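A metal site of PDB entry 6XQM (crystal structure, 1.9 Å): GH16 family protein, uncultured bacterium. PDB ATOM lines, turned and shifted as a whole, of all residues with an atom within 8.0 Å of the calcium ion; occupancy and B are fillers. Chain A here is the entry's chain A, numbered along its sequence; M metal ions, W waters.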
ATOM      1  N   ASP A  30       8.110   9.541  -8.487  1.00  0.00           N
ATOM      2  CA  ASP A  30       7.968  10.253  -7.189  1.00  0.00           C
ATOM      3  C   ASP A  30       7.845   9.184  -6.093  1.00  0.00           C
ATOM      4  O   ASP A  30       6.906   8.362  -6.144  1.00  0.00           O
ATOM      5  CB  ASP A  30       6.873  11.312  -7.265  1.00  0.00           C
ATOM      6  CG  ASP A  30       7.019  12.342  -6.150  1.00  0.00           C
ATOM      7  OD1 ASP A  30       7.783  12.070  -5.164  1.00  0.00           O
ATOM      8  OD2 ASP A  30       6.366  13.364  -6.245  1.00  0.00           O
ATOM      9  N   GLU A  31       8.819   9.199  -5.176  1.00  0.00           N
ATOM     10  CA  GLU A  31       8.928   8.283  -4.019  1.00  0.00           C
ATOM     11  C   GLU A  31       8.164   8.880  -2.825  1.00  0.00           C
ATOM     12  O   GLU A  31       7.961   8.152  -1.853  1.00  0.00           O
ATOM     13  CB  GLU A  31      10.410   8.023  -3.725  1.00  0.00           C
ATOM     14  CG  GLU A  31      11.215   7.283  -4.814  1.00  0.00           C
ATOM     15  CD  GLU A  31      10.639   5.922  -5.102  1.00  0.00           C
ATOM     16  OE1 GLU A  31      10.584   5.523  -6.266  1.00  0.00           O
ATOM     17  OE2 GLU A  31      10.205   5.272  -4.156  1.00  0.00           O
ATOM     18  N   PHE A  32       7.816  10.163  -2.866  1.00  0.00           N
ATOM     19  CA  PHE A  32       7.069  10.896  -1.811  1.00  0.00           C
ATOM     20  C   PHE A  32       7.785  10.769  -0.457  1.00  0.00           C
ATOM     21  O   PHE A  32       7.093  10.625   0.574  1.00  0.00           O
ATOM     22  CB  PHE A  32       5.631  10.390  -1.753  1.00  0.00           C
ATOM     23  CG  PHE A  32       4.853  10.652  -3.006  1.00  0.00           C
ATOM     24  CD1 PHE A  32       4.675  11.953  -3.454  1.00  0.00           C
ATOM     25  CD2 PHE A  32       4.283   9.615  -3.742  1.00  0.00           C
ATOM     26  CE1 PHE A  32       3.956  12.205  -4.632  1.00  0.00           C
ATOM     27  CE2 PHE A  32       3.610   9.877  -4.923  1.00  0.00           C
ATOM     28  CZ  PHE A  32       3.386  11.165  -5.343  1.00  0.00           C
ATOM     29  N   ASN A  33       9.112  10.833  -0.452  1.00  0.00           N
ATOM     30  CA  ASN A  33       9.943  10.712   0.786  1.00  0.00           C
ATOM     31  C   ASN A  33      10.356  12.110   1.286  1.00  0.00           C
ATOM     32  O   ASN A  33      11.207  12.204   2.118  1.00  0.00           O
ATOM     33  CB  ASN A  33      11.099   9.725   0.560  1.00  0.00           C
ATOM     34  CG  ASN A  33      10.581   8.305   0.401  1.00  0.00           C
ATOM     35  OD1 ASN A  33       9.439   7.984   0.740  1.00  0.00           O
ATOM     36  ND2 ASN A  33      11.329   7.461  -0.280  1.00  0.00           N
ATOM     37  N   THR A  34       9.777  13.188   0.772  1.00  0.00           N
ATOM     38  CA  THR A  34      10.055  14.538   1.306  1.00  0.00           C
ATOM     39  C   THR A  34       8.742  15.105   1.825  1.00  0.00           C
ATOM     40  O   THR A  34       7.938  15.609   1.044  1.00  0.00           O
ATOM     41  CB  THR A  34      10.746  15.449   0.296  1.00  0.00           C
ATOM     42  OG1 THR A  34      11.745  14.656  -0.339  1.00  0.00           O
ATOM     43  CG2 THR A  34      11.402  16.651   0.944  1.00  0.00           C
ATOM     44  N   VAL A  72       2.337  15.244   1.600  1.00  0.00           N
ATOM     45  CA  VAL A  72       3.297  14.139   1.747  1.00  0.00           C
ATOM     46  C   VAL A  72       3.728  13.964   3.216  1.00  0.00           C
ATOM     47  O   VAL A  72       4.329  14.887   3.833  1.00  0.00           O
ATOM     48  CB  VAL A  72       4.492  14.386   0.845  1.00  0.00           C
ATOM     49  CG1 VAL A  72       5.418  13.178   0.868  1.00  0.00           C
ATOM     50  CG2 VAL A  72       4.014  14.721  -0.557  1.00  0.00           C
ATOM     51  N   GLU A  73       3.531  12.747   3.749  1.00  0.00           N
ATOM     52  CA  GLU A  73       3.903  12.432   5.155  1.00  0.00           C
ATOM     53  C   GLU A  73       4.226  10.944   5.233  1.00  0.00           C
ATOM     54  O   GLU A  73       3.552  10.139   4.523  1.00  0.00           O
ATOM     55  CB  GLU A  73       2.808  12.935   6.119  1.00  0.00           C
ATOM     56  CG  GLU A  73       1.566  12.070   6.196  1.00  0.00           C
ATOM     57  CD  GLU A  73       0.373  12.611   7.000  1.00  0.00           C
ATOM     58  OE1 GLU A  73       0.507  13.725   7.497  1.00  0.00           O
ATOM     59  OE2 GLU A  73      -0.687  11.874   7.149  1.00  0.00           O
ATOM     60  N   ASN A  74       5.194  10.575   6.075  1.00  0.00           N
ATOM     61  CA  ASN A  74       5.461   9.157   6.407  1.00  0.00           C
ATOM     62  C   ASN A  74       5.723   8.383   5.110  1.00  0.00           C
ATOM     63  O   ASN A  74       5.449   7.197   5.068  1.00  0.00           O
ATOM     64  CB  ASN A  74       4.271   8.529   7.131  1.00  0.00           C
ATOM     65  CG  ASN A  74       3.933   9.234   8.426  1.00  0.00           C
ATOM     66  OD1 ASN A  74       4.844   9.597   9.170  1.00  0.00           O
ATOM     67  ND2 ASN A  74       2.655   9.467   8.684  1.00  0.00           N
ATOM     68  N   GLY A  75       6.242   9.061   4.090  1.00  0.00           N
ATOM     69  CA  GLY A  75       6.756   8.405   2.862  1.00  0.00           C
ATOM     70  C   GLY A  75       5.655   8.147   1.857  1.00  0.00           C
ATOM     71  O   GLY A  75       5.917   7.474   0.833  1.00  0.00           O
ATOM     72  N   ASN A  76       4.482   8.745   2.048  1.00  0.00           N
ATOM     73  CA  ASN A  76       3.355   8.607   1.105  1.00  0.00           C
ATOM     74  C   ASN A  76       2.785   9.957   0.725  1.00  0.00           C
ATOM     75  O   ASN A  76       2.696  10.850   1.609  1.00  0.00           O
ATOM     76  CB  ASN A  76       2.162   7.837   1.683  1.00  0.00           C
ATOM     77  CG  ASN A  76       2.564   6.515   2.293  1.00  0.00           C
ATOM     78  OD1 ASN A  76       3.167   5.671   1.648  1.00  0.00           O
ATOM     79  ND2 ASN A  76       2.202   6.317   3.543  1.00  0.00           N
ATOM     80  N   LEU A  77       2.274  10.058  -0.504  1.00  0.00           N
ATOM     81  CA  LEU A  77       1.310  11.117  -0.832  1.00  0.00           C
ATOM     82  C   LEU A  77      -0.023  10.757  -0.178  1.00  0.00           C
ATOM     83  O   LEU A  77      -0.427   9.596  -0.280  1.00  0.00           O
ATOM     84  CB  LEU A  77       1.154  11.252  -2.338  1.00  0.00           C
ATOM     85  CG  LEU A  77       0.136  12.320  -2.727  1.00  0.00           C
ATOM     86  CD1 LEU A  77       0.726  13.723  -2.557  1.00  0.00           C
ATOM     87  CD2 LEU A  77      -0.397  12.091  -4.157  1.00  0.00           C
ATOM     88  N   ARG A 118       2.011   2.304  -6.274  1.00  0.00           N
ATOM     89  CA  ARG A 118       1.747   1.515  -5.036  1.00  0.00           C
ATOM     90  C   ARG A 118       0.863   2.346  -4.121  1.00  0.00           C
ATOM     91  O   ARG A 118       1.330   3.409  -3.648  1.00  0.00           O
ATOM     92  CB  ARG A 118       3.035   1.013  -4.398  1.00  0.00           C
ATOM     93  CG  ARG A 118       2.822   0.243  -3.098  1.00  0.00           C
ATOM     94  CD  ARG A 118       4.009  -0.623  -2.671  1.00  0.00           C
ATOM     95  NE  ARG A 118       3.754  -1.383  -1.423  1.00  0.00           N
ATOM     96  CZ  ARG A 118       3.905  -0.932  -0.148  1.00  0.00           C
ATOM     97  NH1 ARG A 118       4.372   0.263   0.150  1.00  0.00           N
ATOM     98  NH2 ARG A 118       3.588  -1.744   0.866  1.00  0.00           N
ATOM     99  N   PHE A 191      -1.470  -1.898   1.217  1.00  0.00           N
ATOM    100  CA  PHE A 191      -0.980  -1.413  -0.096  1.00  0.00           C
ATOM    101  C   PHE A 191      -1.084  -2.526  -1.134  1.00  0.00           C
ATOM    102  O   PHE A 191      -0.930  -3.738  -0.812  1.00  0.00           O
ATOM    103  CB  PHE A 191       0.454  -0.917   0.013  1.00  0.00           C
ATOM    104  CG  PHE A 191       0.543   0.417   0.696  1.00  0.00           C
ATOM    105  CD1 PHE A 191       0.561   0.498   2.079  1.00  0.00           C
ATOM    106  CD2 PHE A 191       0.529   1.575  -0.040  1.00  0.00           C
ATOM    107  CE1 PHE A 191       0.658   1.724   2.702  1.00  0.00           C
ATOM    108  CE2 PHE A 191       0.591   2.805   0.596  1.00  0.00           C
ATOM    109  CZ  PHE A 191       0.667   2.885   1.957  1.00  0.00           C
ATOM    110  N   VAL A 260      -0.355   7.093  -1.327  1.00  0.00           N
ATOM    111  CA  VAL A 260       0.451   6.632  -2.495  1.00  0.00           C
ATOM    112  C   VAL A 260       1.902   6.574  -2.044  1.00  0.00           C
ATOM    113  O   VAL A 260       2.473   7.624  -1.709  1.00  0.00           O
ATOM    114  CB  VAL A 260       0.257   7.514  -3.740  1.00  0.00           C
ATOM    115  CG1 VAL A 260       1.019   6.959  -4.929  1.00  0.00           C
ATOM    116  CG2 VAL A 260      -1.205   7.673  -4.073  1.00  0.00           C
ATOM    117  N   ASP A 261       2.440   5.363  -2.007  1.00  0.00           N
ATOM    118  CA  ASP A 261       3.836   5.104  -1.576  1.00  0.00           C
ATOM    119  C   ASP A 261       4.756   5.670  -2.667  1.00  0.00           C
ATOM    120  O   ASP A 261       5.725   6.361  -2.371  1.00  0.00           O
ATOM    121  CB  ASP A 261       4.085   3.630  -1.266  1.00  0.00           C
ATOM    122  CG  ASP A 261       5.469   3.383  -0.694  1.00  0.00           C
ATOM    123  OD1 ASP A 261       6.144   4.373  -0.322  1.00  0.00           O
ATOM    124  OD2 ASP A 261       5.887   2.240  -0.706  1.00  0.00           O
ATOM    125  N   TYR A 262       4.456   5.360  -3.900  1.00  0.00           N
ATOM    126  CA  TYR A 262       5.294   5.863  -4.995  1.00  0.00           C
ATOM    127  C   TYR A 262       4.585   5.753  -6.320  1.00  0.00           C
ATOM    128  O   TYR A 262       3.685   4.928  -6.516  1.00  0.00           O
ATOM    129  CB  TYR A 262       6.631   5.111  -5.012  1.00  0.00           C
ATOM    130  CG  TYR A 262       6.523   3.627  -5.217  1.00  0.00           C
ATOM    131  CD1 TYR A 262       6.119   3.092  -6.422  1.00  0.00           C
ATOM    132  CD2 TYR A 262       6.878   2.737  -4.205  1.00  0.00           C
ATOM    133  CE1 TYR A 262       6.077   1.727  -6.625  1.00  0.00           C
ATOM    134  CE2 TYR A 262       6.847   1.372  -4.400  1.00  0.00           C
ATOM    135  CZ  TYR A 262       6.452   0.868  -5.618  1.00  0.00           C
ATOM    136  OH  TYR A 262       6.392  -0.490  -5.833  1.00  0.00           O
ATOM    137  N   VAL A 263       5.101   6.549  -7.238  1.00  0.00           N
ATOM    138  CA  VAL A 263       4.832   6.412  -8.679  1.00  0.00           C
ATOM    139  C   VAL A 263       6.167   6.136  -9.382  1.00  0.00           C
ATOM    140  O   VAL A 263       7.073   6.956  -9.207  1.00  0.00           O
ATOM    141  CB  VAL A 263       4.181   7.666  -9.289  1.00  0.00           C
ATOM    142  CG1 VAL A 263       4.113   7.552 -10.797  1.00  0.00           C
ATOM    143  CG2 VAL A 263       2.810   7.950  -8.683  1.00  0.00           C
ATOM    144  N   ARG A 264       6.215   5.113 -10.216  1.00  0.00           N
ATOM    145  CA  ARG A 264       7.421   4.844 -11.019  1.00  0.00           C
ATOM    146  C   ARG A 264       6.997   4.619 -12.471  1.00  0.00           C
ATOM    147  O   ARG A 264       6.078   3.812 -12.714  1.00  0.00           O
ATOM    148  CB  ARG A 264       8.182   3.666 -10.432  1.00  0.00           C
ATOM    149  CG  ARG A 264       8.739   3.894  -9.048  1.00  0.00           C
ATOM    150  CD  ARG A 264       9.394   2.655  -8.507  1.00  0.00           C
ATOM    151  NE  ARG A 264       9.664   2.851  -7.092  1.00  0.00           N
ATOM    152  CZ  ARG A 264       9.867   1.886  -6.220  1.00  0.00           C
ATOM    153  NH1 ARG A 264       9.867   0.621  -6.598  1.00  0.00           N
ATOM    154  NH2 ARG A 264      10.103   2.195  -4.958  1.00  0.00           N
HETATM  155 CA    CA M   1       7.350   6.371  -0.566  1.00  0.00          CA
HETATM  156  O   HOH W   1       8.972   5.001  -1.864  1.00  0.00           O
HETATM  157  O   HOH W   2       8.344   5.197   1.465  1.00  0.00           O
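The calcium ion is bound by O of Glu 31 (2.3 Å), O of Gly 75 (2.3 Å), OD1 of Asp 261 (2.3 Å), O of Asp 261 (2.4 Å), water W1 (2.5 Å) and water W2 (2.5 Å). The calcium ion has six donor atoms within binding distance. Slightly farther from the calcium ion lies OD1 of Asn 33 (2.9 Å).
NH1 of Arg 118 lies within salt-bridge range of OD2 of Asp 261 (2.6 Å). The side-chain amide oxygen (OD1) of Asn 33 sits close to the backbone carbonyl oxygen (O) of Glu 31. OE1 of Glu 31 is in salt-bridge range of NE of Arg 264, 2.9 Å away.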
